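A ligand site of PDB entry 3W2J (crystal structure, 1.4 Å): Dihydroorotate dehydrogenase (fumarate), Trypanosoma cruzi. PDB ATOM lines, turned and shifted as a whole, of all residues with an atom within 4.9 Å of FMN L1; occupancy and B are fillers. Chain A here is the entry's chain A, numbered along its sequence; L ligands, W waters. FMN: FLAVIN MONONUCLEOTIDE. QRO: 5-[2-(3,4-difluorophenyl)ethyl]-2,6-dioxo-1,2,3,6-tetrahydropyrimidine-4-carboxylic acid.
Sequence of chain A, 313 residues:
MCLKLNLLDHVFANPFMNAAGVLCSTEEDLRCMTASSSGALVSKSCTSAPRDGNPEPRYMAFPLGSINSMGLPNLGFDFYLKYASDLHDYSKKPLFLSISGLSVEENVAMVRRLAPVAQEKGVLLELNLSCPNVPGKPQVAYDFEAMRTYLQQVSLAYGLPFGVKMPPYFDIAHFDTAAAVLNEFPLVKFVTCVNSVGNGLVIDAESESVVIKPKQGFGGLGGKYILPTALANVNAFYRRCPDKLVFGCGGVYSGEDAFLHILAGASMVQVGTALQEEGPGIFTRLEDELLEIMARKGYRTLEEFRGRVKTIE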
ATOM      1  N   ALA A  19      18.354   6.763 -27.961  1.00  0.00           N
ATOM      2  CA  ALA A  19      18.545   6.382 -26.590  1.00  0.00           C
ATOM      3  C   ALA A  19      19.221   7.482 -25.801  1.00  0.00           C
ATOM      4  O   ALA A  19      20.124   8.158 -26.354  1.00  0.00           O
ATOM      5  CB  ALA A  19      19.353   5.109 -26.488  1.00  0.00           C
ATOM      6  N   ALA A  20      18.879   7.759 -24.555  1.00  0.00           N
ATOM      7  CA  ALA A  20      19.497   8.802 -23.816  1.00  0.00           C
ATOM      8  C   ALA A  20      20.986   8.585 -23.818  1.00  0.00           C
ATOM      9  O   ALA A  20      21.533   7.471 -23.691  1.00  0.00           O
ATOM     10  CB  ALA A  20      18.938   8.884 -22.389  1.00  0.00           C
ATOM     11  N   GLY A  21      21.749   9.665 -23.977  1.00  0.00           N
ATOM     12  CA  GLY A  21      23.171   9.717 -24.040  1.00  0.00           C
ATOM     13  C   GLY A  21      23.749   9.750 -25.411  1.00  0.00           C
ATOM     14  O   GLY A  21      24.898  10.144 -25.590  1.00  0.00           O
ATOM     15  N   VAL A  22      22.999   9.325 -26.432  1.00  0.00           N
ATOM     16  CA  VAL A  22      23.553   9.301 -27.804  1.00  0.00           C
ATOM     17  C   VAL A  22      22.908  10.467 -28.559  1.00  0.00           C
ATOM     18  O   VAL A  22      21.679  10.598 -28.630  1.00  0.00           O
ATOM     19  CB  VAL A  22      23.239   7.921 -28.439  1.00  0.00           C
ATOM     20  CG1 VAL A  22      23.639   7.940 -29.903  1.00  0.00           C
ATOM     21  CG2 VAL A  22      23.943   6.879 -27.619  1.00  0.00           C
ATOM     22  N   LYS A  44      20.255  14.182 -23.117  1.00  0.00           N
ATOM     23  CA  LYS A  44      21.237  13.556 -22.297  1.00  0.00           C
ATOM     24  C   LYS A  44      20.856  13.595 -20.812  1.00  0.00           C
ATOM     25  O   LYS A  44      20.503  14.693 -20.355  1.00  0.00           O
ATOM     26  CB  LYS A  44      22.600  14.232 -22.501  1.00  0.00           C
ATOM     27  CG  LYS A  44      23.700  13.773 -21.554  1.00  0.00           C
ATOM     28  CD  LYS A  44      24.221  12.280 -21.699  1.00  0.00           C
ATOM     29  CE  LYS A  44      25.041  11.767 -20.505  1.00  0.00           C
ATOM     30  NZ  LYS A  44      25.581  10.286 -20.646  1.00  0.00           N
ATOM     31  N   SER A  45      20.999  12.486 -20.143  1.00  0.00           N
ATOM     32  CA  SER A  45      20.692  12.469 -18.698  1.00  0.00           C
ATOM     33  C   SER A  45      21.556  13.542 -18.025  1.00  0.00           C
ATOM     34  O   SER A  45      22.754  13.636 -18.229  1.00  0.00           O
ATOM     35  CB  SER A  45      21.059  11.187 -18.041  1.00  0.00           C
ATOM     36  OG  SER A  45      20.209  10.153 -18.517  1.00  0.00           O
ATOM     37  N   TYR A  59      34.346   5.588 -24.479  1.00  0.00           N
ATOM     38  CA  TYR A  59      33.394   4.866 -25.338  1.00  0.00           C
ATOM     39  C   TYR A  59      34.182   4.209 -26.432  1.00  0.00           C
ATOM     40  O   TYR A  59      35.040   4.858 -27.056  1.00  0.00           O
ATOM     41  CB  TYR A  59      32.373   5.845 -25.971  1.00  0.00           C
ATOM     42  CG  TYR A  59      31.489   5.213 -27.069  1.00  0.00           C
ATOM     43  CD1 TYR A  59      30.337   4.507 -26.770  1.00  0.00           C
ATOM     44  CD2 TYR A  59      31.905   5.307 -28.381  1.00  0.00           C
ATOM     45  CE1 TYR A  59      29.590   3.912 -27.755  1.00  0.00           C
ATOM     46  CE2 TYR A  59      31.175   4.653 -29.347  1.00  0.00           C
ATOM     47  CZ  TYR A  59      29.992   3.980 -29.079  1.00  0.00           C
ATOM     48  OH  TYR A  59      29.187   3.407 -30.028  1.00  0.00           O
ATOM     49  N   SER A  66      29.032  -1.963 -28.177  1.00  0.00           N
ATOM     50  CA  SER A  66      29.815  -0.906 -27.595  1.00  0.00           C
ATOM     51  C   SER A  66      29.993  -1.143 -26.116  1.00  0.00           C
ATOM     52  O   SER A  66      29.274  -1.881 -25.451  1.00  0.00           O
ATOM     53  CB  SER A  66      29.179   0.446 -27.817  1.00  0.00           C
ATOM     54  OG  SER A  66      27.955   0.570 -27.061  1.00  0.00           O
ATOM     55  N   ASN A  68      30.932   1.512 -22.633  1.00  0.00           N
ATOM     56  CA  ASN A  68      31.114   2.916 -22.207  1.00  0.00           C
ATOM     57  C   ASN A  68      31.163   3.041 -20.709  1.00  0.00           C
ATOM     58  O   ASN A  68      30.453   2.420 -19.948  1.00  0.00           O
ATOM     59  CB  ASN A  68      30.069   3.896 -22.795  1.00  0.00           C
ATOM     60  CG  ASN A  68      28.827   3.955 -21.954  1.00  0.00           C
ATOM     61  OD1 ASN A  68      28.764   4.722 -20.963  1.00  0.00           O
ATOM     62  ND2 ASN A  68      27.811   3.204 -22.289  1.00  0.00           N
ATOM     63  N   MET A  70      31.102   6.671 -19.536  1.00  0.00           N
ATOM     64  CA  MET A  70      31.210   8.086 -19.862  1.00  0.00           C
ATOM     65  C   MET A  70      31.404   8.949 -18.622  1.00  0.00           C
ATOM     66  O   MET A  70      32.026   9.993 -18.677  1.00  0.00           O
ATOM     67  CB  MET A  70      29.946   8.525 -20.548  1.00  0.00           C
ATOM     68  CG  MET A  70      29.592   7.859 -21.856  1.00  0.00           C
ATOM     69  SD  MET A  70      30.882   7.926 -23.119  1.00  0.00           S
ATOM     70  CE  MET A  70      30.821   9.538 -23.606  1.00  0.00           C
ATOM     71  N   LEU A  72      28.688  10.356 -16.966  1.00  0.00           N
ATOM     72  CA  LEU A  72      27.646  11.312 -17.004  1.00  0.00           C
ATOM     73  C   LEU A  72      28.088  12.713 -17.413  1.00  0.00           C
ATOM     74  O   LEU A  72      27.651  13.712 -16.802  1.00  0.00           O
ATOM     75  CB  LEU A  72      26.877  11.260 -15.688  1.00  0.00           C
ATOM     76  CG  LEU A  72      25.460  11.665 -15.447  1.00  0.00           C
ATOM     77  CD1 LEU A  72      24.555  11.233 -16.537  1.00  0.00           C
ATOM     78  CD2 LEU A  72      25.068  11.047 -14.104  1.00  0.00           C
ATOM     79  N   SER A  98      15.752  13.550 -19.927  1.00  0.00           N
ATOM     80  CA  SER A  98      16.216  12.544 -19.003  1.00  0.00           C
ATOM     81  C   SER A  98      16.992  13.182 -17.860  1.00  0.00           C
ATOM     82  O   SER A  98      17.816  14.099 -18.082  1.00  0.00           O
ATOM     83  CB  SER A  98      17.152  11.548 -19.721  1.00  0.00           C
ATOM     84  OG  SER A  98      17.676  10.633 -18.760  1.00  0.00           O
ATOM     85  N   GLU A 126      11.929  11.397 -18.412  1.00  0.00           N
ATOM     86  CA  GLU A 126      12.486  10.038 -18.229  1.00  0.00           C
ATOM     87  C   GLU A 126      13.480  10.093 -17.095  1.00  0.00           C
ATOM     88  O   GLU A 126      14.550  10.662 -17.206  1.00  0.00           O
ATOM     89  CB  GLU A 126      13.100   9.491 -19.530  1.00  0.00           C
ATOM     90  CG  GLU A 126      13.559   8.033 -19.434  1.00  0.00           C
ATOM     91  CD  GLU A 126      14.137   7.461 -20.751  1.00  0.00           C
ATOM     92  OE1 GLU A 126      15.340   7.609 -20.938  1.00  0.00           O
ATOM     93  OE2 GLU A 126      13.421   6.801 -21.569  1.00  0.00           O
ATOM     94  N   ASN A 128      16.223   8.386 -14.937  1.00  0.00           N
ATOM     95  CA  ASN A 128      17.195   7.317 -15.031  1.00  0.00           C
ATOM     96  C   ASN A 128      17.518   6.701 -13.659  1.00  0.00           C
ATOM     97  O   ASN A 128      18.134   7.274 -12.899  1.00  0.00           O
ATOM     98  CB  ASN A 128      18.470   7.873 -15.649  1.00  0.00           C
ATOM     99  CG  ASN A 128      19.507   6.821 -15.924  1.00  0.00           C
ATOM    100  OD1 ASN A 128      19.309   5.687 -15.800  1.00  0.00           O
ATOM    101  ND2 ASN A 128      20.611   7.273 -16.399  1.00  0.00           N
ATOM    102  N   LYS A 165      13.795   4.878 -16.733  1.00  0.00           N
ATOM    103  CA  LYS A 165      14.801   4.101 -17.505  1.00  0.00           C
ATOM    104  C   LYS A 165      15.371   3.076 -16.564  1.00  0.00           C
ATOM    105  O   LYS A 165      15.944   3.397 -15.504  1.00  0.00           O
ATOM    106  CB  LYS A 165      15.877   4.985 -18.025  1.00  0.00           C
ATOM    107  CG  LYS A 165      16.979   4.365 -18.860  1.00  0.00           C
ATOM    108  CD  LYS A 165      16.590   3.854 -20.210  1.00  0.00           C
ATOM    109  CE  LYS A 165      17.750   3.494 -21.095  1.00  0.00           C
ATOM    110  NZ  LYS A 165      18.556   4.648 -21.529  1.00  0.00           N
ATOM    111  N   VAL A 194      16.053  -1.353 -22.101  1.00  0.00           N
ATOM    112  CA  VAL A 194      16.971  -1.337 -20.919  1.00  0.00           C
ATOM    113  C   VAL A 194      18.114  -0.357 -21.173  1.00  0.00           C
ATOM    114  O   VAL A 194      18.470   0.024 -22.329  1.00  0.00           O
ATOM    115  CB  VAL A 194      17.591  -2.764 -20.643  1.00  0.00           C
ATOM    116  CG1 VAL A 194      16.523  -3.752 -20.246  1.00  0.00           C
ATOM    117  CG2 VAL A 194      18.356  -3.280 -21.889  1.00  0.00           C
ATOM    118  N   ASN A 195      18.693   0.029 -20.075  1.00  0.00           N
ATOM    119  CA  ASN A 195      20.003   0.625 -19.987  1.00  0.00           C
ATOM    120  C   ASN A 195      21.065  -0.438 -20.327  1.00  0.00           C
ATOM    121  O   ASN A 195      20.746  -1.533 -20.576  1.00  0.00           O
ATOM    122  CB  ASN A 195      20.240   1.334 -18.608  1.00  0.00           C
ATOM    123  CG  ASN A 195      21.096   2.615 -18.731  1.00  0.00           C
ATOM    124  OD1 ASN A 195      22.120   2.617 -19.330  1.00  0.00           O
ATOM    125  ND2 ASN A 195      20.628   3.680 -18.122  1.00  0.00           N
ATOM    126  N   SER A 196      22.299   0.009 -20.305  1.00  0.00           N
ATOM    127  CA  SER A 196      23.346  -0.927 -20.651  1.00  0.00           C
ATOM    128  C   SER A 196      23.481  -2.117 -19.718  1.00  0.00           C
ATOM    129  O   SER A 196      23.124  -2.082 -18.609  1.00  0.00           O
ATOM    130  CB  SER A 196      24.684  -0.212 -20.855  1.00  0.00           C
ATOM    131  OG  SER A 196      24.926   0.765 -20.025  1.00  0.00           O
ATOM    132  N   GLY A 222      26.349  -2.156 -24.813  1.00  0.00           N
ATOM    133  CA  GLY A 222      25.248  -1.969 -25.726  1.00  0.00           C
ATOM    134  C   GLY A 222      25.372  -2.685 -27.017  1.00  0.00           C
ATOM    135  O   GLY A 222      26.468  -3.243 -27.291  1.00  0.00           O
ATOM    136  N   GLY A 223      24.361  -2.702 -27.849  1.00  0.00           N
ATOM    137  CA  GLY A 223      24.445  -3.205 -29.126  1.00  0.00           C
ATOM    138  C   GLY A 223      24.027  -4.642 -29.328  1.00  0.00           C
ATOM    139  O   GLY A 223      23.169  -5.134 -28.573  1.00  0.00           O
ATOM    140  N   ILE A 226      23.373  -7.332 -26.543  1.00  0.00           N
ATOM    141  CA  ILE A 226      22.362  -7.192 -25.520  1.00  0.00           C
ATOM    142  C   ILE A 226      20.907  -7.353 -26.034  1.00  0.00           C
ATOM    143  O   ILE A 226      19.984  -7.254 -25.233  1.00  0.00           O
ATOM    144  CB  ILE A 226      22.465  -5.855 -24.725  1.00  0.00           C
ATOM    145  CG1 ILE A 226      21.909  -4.618 -25.423  1.00  0.00           C
ATOM    146  CG2 ILE A 226      23.897  -5.689 -24.248  1.00  0.00           C
ATOM    147  CD1 ILE A 226      21.660  -3.499 -24.446  1.00  0.00           C
ATOM    148  N   CYS A 249      14.633  -0.525 -25.616  1.00  0.00           N
ATOM    149  CA  CYS A 249      15.972  -0.017 -25.935  1.00  0.00           C
ATOM    150  C   CYS A 249      16.942  -1.195 -25.762  1.00  0.00           C
ATOM    151  O   CYS A 249      16.898  -1.900 -24.791  1.00  0.00           O
ATOM    152  CB  CYS A 249      16.333   1.093 -25.016  1.00  0.00           C
ATOM    153  SG  CYS A 249      17.853   1.953 -25.396  1.00  0.00           S
ATOM    154  N   GLY A 250      17.746  -1.384 -26.769  1.00  0.00           N
ATOM    155  CA  GLY A 250      18.874  -2.348 -26.710  1.00  0.00           C
ATOM    156  C   GLY A 250      18.972  -3.193 -27.944  1.00  0.00           C
ATOM    157  O   GLY A 250      18.049  -3.918 -28.289  1.00  0.00           O
ATOM    158  N   GLY A 251      20.113  -3.081 -28.617  1.00  0.00           N
ATOM    159  CA  GLY A 251      20.370  -3.937 -29.749  1.00  0.00           C
ATOM    160  C   GLY A 251      19.586  -3.681 -30.963  1.00  0.00           C
ATOM    161  O   GLY A 251      19.615  -4.526 -31.884  1.00  0.00           O
ATOM    162  N   VAL A 252      19.068  -2.465 -31.134  1.00  0.00           N
ATOM    163  CA  VAL A 252      18.344  -2.161 -32.400  1.00  0.00           C
ATOM    164  C   VAL A 252      19.307  -1.634 -33.432  1.00  0.00           C
ATOM    165  O   VAL A 252      19.836  -0.556 -33.306  1.00  0.00           O
ATOM    166  CB  VAL A 252      17.163  -1.160 -32.165  1.00  0.00           C
ATOM    167  CG1 VAL A 252      16.478  -0.792 -33.510  1.00  0.00           C
ATOM    168  CG2 VAL A 252      16.167  -1.722 -31.180  1.00  0.00           C
ATOM    169  N   GLN A 270      13.953   2.822 -28.875  1.00  0.00           N
ATOM    170  CA  GLN A 270      15.098   3.720 -28.780  1.00  0.00           C
ATOM    171  C   GLN A 270      16.367   3.016 -29.371  1.00  0.00           C
ATOM    172  O   GLN A 270      16.501   1.844 -29.297  1.00  0.00           O
ATOM    173  CB  GLN A 270      15.399   4.103 -27.326  1.00  0.00           C
ATOM    174  CG  GLN A 270      14.163   4.489 -26.503  1.00  0.00           C
ATOM    175  CD  GLN A 270      14.553   5.072 -25.169  1.00  0.00           C
ATOM    176  OE1 GLN A 270      15.516   4.711 -24.615  1.00  0.00           O
ATOM    177  NE2 GLN A 270      13.709   5.870 -24.649  1.00  0.00           N
ATOM    178  N   VAL A 271      17.252   3.869 -29.934  1.00  0.00           N
ATOM    179  CA  VAL A 271      18.438   3.436 -30.652  1.00  0.00           C
ATOM    180  C   VAL A 271      19.650   4.112 -30.108  1.00  0.00           C
ATOM    181  O   VAL A 271      19.732   5.361 -30.168  1.00  0.00           O
ATOM    182  CB  VAL A 271      18.238   3.734 -32.131  1.00  0.00           C
ATOM    183  CG1 VAL A 271      19.361   3.085 -32.896  1.00  0.00           C
ATOM    184  CG2 VAL A 271      16.866   3.252 -32.669  1.00  0.00           C
ATOM    185  N   GLY A 272      20.584   3.342 -29.514  1.00  0.00           N
ATOM    186  CA  GLY A 272      21.805   3.854 -28.902  1.00  0.00           C
ATOM    187  C   GLY A 272      23.003   3.638 -29.812  1.00  0.00           C
ATOM    188  O   GLY A 272      23.322   4.401 -30.680  1.00  0.00           O
ATOM    189  N   THR A 273      23.688   2.534 -29.507  1.00  0.00           N
ATOM    190  CA  THR A 273      24.924   2.141 -30.226  1.00  0.00           C
ATOM    191  C   THR A 273      24.822   2.297 -31.721  1.00  0.00           C
ATOM    192  O   THR A 273      25.684   2.874 -32.348  1.00  0.00           O
ATOM    193  CB  THR A 273      25.321   0.716 -29.849  1.00  0.00           C
ATOM    194  OG1 THR A 273      25.577   0.624 -28.447  1.00  0.00           O
ATOM    195  CG2 THR A 273      26.591   0.300 -30.527  1.00  0.00           C
ATOM    196  N   ALA A 274      23.760   1.743 -32.301  1.00  0.00           N
ATOM    197  CA  ALA A 274      23.688   1.760 -33.745  1.00  0.00           C
ATOM    198  C   ALA A 274      23.582   3.169 -34.308  1.00  0.00           C
ATOM    199  O   ALA A 274      24.077   3.494 -35.394  1.00  0.00           O
ATOM    200  CB  ALA A 274      22.487   0.923 -34.262  1.00  0.00           C
HETATM  201  N1  FMN L   1      21.367   5.812 -20.744  1.00  0.00           N
HETATM  202  C2  FMN L   1      20.763   6.801 -20.007  1.00  0.00           C
HETATM  203  O2  FMN L   1      19.629   6.571 -19.570  1.00  0.00           O
HETATM  204  N3  FMN L   1      21.356   8.000 -19.794  1.00  0.00           N
HETATM  205  C4  FMN L   1      22.564   8.307 -20.313  1.00  0.00           C
HETATM  206  O4  FMN L   1      22.992   9.480 -20.138  1.00  0.00           O
HETATM  207  C4A FMN L   1      23.243   7.393 -21.101  1.00  0.00           C
HETATM  208  N5  FMN L   1      24.450   7.634 -21.677  1.00  0.00           N
HETATM  209  C5A FMN L   1      24.911   6.805 -22.617  1.00  0.00           C
HETATM  210  C6  FMN L   1      26.083   7.145 -23.314  1.00  0.00           C
HETATM  211  C7  FMN L   1      26.552   6.352 -24.328  1.00  0.00           C
HETATM  212  C7M FMN L   1      27.794   6.786 -25.139  1.00  0.00           C
HETATM  213  C8  FMN L   1      25.953   5.114 -24.601  1.00  0.00           C
HETATM  214  C8M FMN L   1      26.443   4.157 -25.668  1.00  0.00           C
HETATM  215  C9  FMN L   1      24.851   4.740 -23.885  1.00  0.00           C
HETATM  216  C9A FMN L   1      24.295   5.554 -22.904  1.00  0.00           C
HETATM  217  N10 FMN L   1      23.130   5.217 -22.144  1.00  0.00           N
HETATM  218  C10 FMN L   1      22.545   6.167 -21.348  1.00  0.00           C
HETATM  219  C1' FMN L   1      22.484   3.913 -22.402  1.00  0.00           C
HETATM  220  C2' FMN L   1      21.648   3.922 -23.680  1.00  0.00           C
HETATM  221  O2' FMN L   1      20.560   4.870 -23.500  1.00  0.00           O
HETATM  222  C3' FMN L   1      21.031   2.601 -23.950  1.00  0.00           C
HETATM  223  O3' FMN L   1      20.199   2.259 -22.841  1.00  0.00           O
HETATM  224  C4' FMN L   1      22.091   1.444 -24.076  1.00  0.00           C
HETATM  225  O4' FMN L   1      23.180   1.962 -24.891  1.00  0.00           O
HETATM  226  C5' FMN L   1      21.496   0.257 -24.828  1.00  0.00           C
HETATM  227  O5' FMN L   1      20.977   0.517 -26.102  1.00  0.00           O
HETATM  228  P   FMN L   1      21.799   0.125 -27.439  1.00  0.00           P
HETATM  229  O1P FMN L   1      20.937   0.672 -28.584  1.00  0.00           O
HETATM  230  O2P FMN L   1      21.993  -1.351 -27.437  1.00  0.00           O
HETATM  231  O3P FMN L   1      23.168   0.860 -27.337  1.00  0.00           O
HETATM  232  OAA QRO L   2      28.397   6.370 -18.007  1.00  0.00           O
HETATM  233  CAN QRO L   2      27.474   7.160 -18.269  1.00  0.00           C
HETATM  234  OAD QRO L   2      27.232   8.397 -18.499  1.00  0.00           O
HETATM  235  CAR QRO L   2      26.135   6.299 -18.538  1.00  0.00           C
HETATM  236  NAL QRO L   2      26.278   5.280 -19.518  1.00  0.00           N
HETATM  237  CAT QRO L   2      25.323   4.380 -19.763  1.00  0.00           C
HETATM  238  OAB QRO L   2      25.503   3.458 -20.578  1.00  0.00           O
HETATM  239  NAM QRO L   2      24.148   4.527 -19.121  1.00  0.00           N
HETATM  240  CAU QRO L   2      23.862   5.518 -18.173  1.00  0.00           C
HETATM  241  OAC QRO L   2      22.766   5.598 -17.609  1.00  0.00           O
HETATM  242  CAS QRO L   2      24.931   6.417 -17.900  1.00  0.00           C
HETATM  243  CAK QRO L   2      24.769   7.457 -16.895  1.00  0.00           C
HETATM  244  CAJ QRO L   2      24.782   6.817 -15.441  1.00  0.00           C
HETATM  245  CAO QRO L   2      25.929   6.149 -15.012  1.00  0.00           C
HETATM  246  CAI QRO L   2      26.092   4.738 -15.178  1.00  0.00           C
HETATM  247  CAQ QRO L   2      27.280   4.059 -14.789  1.00  0.00           C
HETATM  248  FAF QRO L   2      27.443   2.721 -15.003  1.00  0.00           F
HETATM  249  CAP QRO L   2      28.322   4.770 -14.259  1.00  0.00           C
HETATM  250  FAE QRO L   2      29.472   4.034 -13.905  1.00  0.00           F
HETATM  251  CAH QRO L   2      28.235   6.133 -14.080  1.00  0.00           C
HETATM  252  CAG QRO L   2      27.064   6.881 -14.419  1.00  0.00           C
HETATM  253  O   HOH W   1      18.491  -0.175 -29.215  1.00  0.00           O
HETATM  254  O   HOH W   2      21.731   0.113 -31.130  1.00  0.00           O
HETATM  255  O   HOH W   3      25.280   1.033 -23.340  1.00  0.00           O
HETATM  256  O   HOH W   4      17.256   8.085 -19.080  1.00  0.00           O
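N of Thr 273 lies within hydrogen-bond range of O3P of FMN L1, 2.8 Å away.
The side-chain hydroxyl (OG1) of Thr 273 is in hydrogen-bond range of an oxygen (O3P) of FMN L1.
The side-chain hydroxyl of Ser 45 lies within hydrogen-bond range of a nitrogen (N3) of FMN L1.
N of Gly 223 lies within hydrogen-bond range of O2P of FMN L1 (2.8 Å).
O4 of FMN L1 sits at hydrogen-bond distance from NZ of Lys 44.
O of Ala 20 sits at hydrogen-bond distance from O2' of FMN L1 (2.8 Å).
The backbone NH (N) of Gly 251 lies within hydrogen-bond range of an oxygen (O2P) of FMN L1 (2.8 Å).
NZ of Lys 165 is in hydrogen-bond range of O2' of FMN L1, 2.8 Å away.
O1P of FMN L1 is in hydrogen-bond range of N of Gly 272, at 2.8 Å.
The backbone carbonyl oxygen (O) of Val 194 is in hydrogen-bond range of an oxygen (O3') of FMN L1 (2.9 Å).
The side-chain amide nitrogen of Asn 195 is in hydrogen-bond range of an oxygen (O2) of FMN L1, 3.4 Å away.
ND2 of Asn 128 sits at hydrogen-bond distance from O2 of FMN L1 (3.4 Å).
The side-chain sulfur of Cys 249 lies within hydrogen-bond range of an oxygen (O3') of FMN L1 (3.5 Å).
The side-chain amino group of Lys 44 is in salt-bridge range of an oxygen (OAD) of QRO L2 (3.3 Å).
The side-chain amide oxygen of Asn 195 sits at hydrogen-bond distance from a nitrogen (NAM) of QRO L2 (2.8 Å).
The side-chain amide nitrogen of Asn 128 lies within hydrogen-bond range of an oxygen (OAC) of QRO L2.
The side-chain amide nitrogen of Asn 68 is in hydrogen-bond range of an oxygen (OAB) of QRO L2.
N of Met 70 is in hydrogen-bond range of OAA of QRO L2, at 3.1 Å.
OG of Ser 196 sits at hydrogen-bond distance from OAB of QRO L2 (2.8 Å).
The backbone NH (N) of Leu 72 is in hydrogen-bond range of an oxygen (OAD) of QRO L2.
N1 of FMN L1 sits close to NAM of QRO L2, 3.5 Å away.
The side-chain hydroxyl (OG) of Ser 66 sits at hydrogen-bond distance from the side-chain hydroxyl (OG1) of Thr 273 (2.8 Å).
OG of Ser 98 sits at hydrogen-bond distance from OG of Ser 45 (2.6 Å).
The backbone NH (N) of Val 194 sits at hydrogen-bond distance from the backbone carbonyl oxygen (O) of Cys 249, 2.9 Å away.
The side-chain amide nitrogen of Asn 195 lies within hydrogen-bond range of the side-chain amide oxygen of Asn 128.
OG of Ser 196 sits at hydrogen-bond distance from OD1 of Asn 195.
The side-chain sulfur (SG) of Cys 249 sits at hydrogen-bond distance from the side-chain amide oxygen (OE1) of Gln 270 (3.7 Å).
N of Met 70 sits at hydrogen-bond distance from OD1 of Asn 68.
The backbone NH (N) of Ser 66 is in hydrogen-bond range of the backbone carbonyl oxygen (O) of Gly 222 (3.0 Å).
Residues that only touch FMN L1: Ala 19, Gly 250, Gly 21, Asn 68, Gly 222, Ile 226, Tyr 59, Met 70, Val 271 and Ser 196.
Hydrophobic or aromatic side chains within 4 Å of FMN L1: Ala 19, Ala 20, Tyr 59, Met 70 and Ile 226.
Within 4 Å of FMN L1: Ala 19, Ala 20, Gly 21, Lys 44, Ser 45, Tyr 59, Asn 68, Met 70, Asn 128, Lys 165, Val 194, Asn 195, Ser 196, Gly 222, Gly 223, Ile 226, Cys 249, Gly 250, Gly 251, Val 271, Gly 272 and Thr 273.
The nearest printed residue that does not touch FMN L1 is Val 22 (4.03 Å).
Water W2 lies within hydrogen-bond range of O1P of FMN L1 (2.7 Å), N of Ala 274 (2.9 Å) and O of Val 252 (3.0 Å).
Water W3 lies within hydrogen-bond range of O4' of FMN L1 (2.8 Å), OG of Ser 196 (3.3 Å) and ND2 of Asn 68 (3.5 Å).
Water W4 lies within hydrogen-bond range of the side-chain hydroxyl (OG) of Ser 98 (2.6 Å), the side-chain carboxylate (OE1) of Glu 126 (2.7 Å) and an oxygen (O2) of FMN L1 (2.9 Å).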
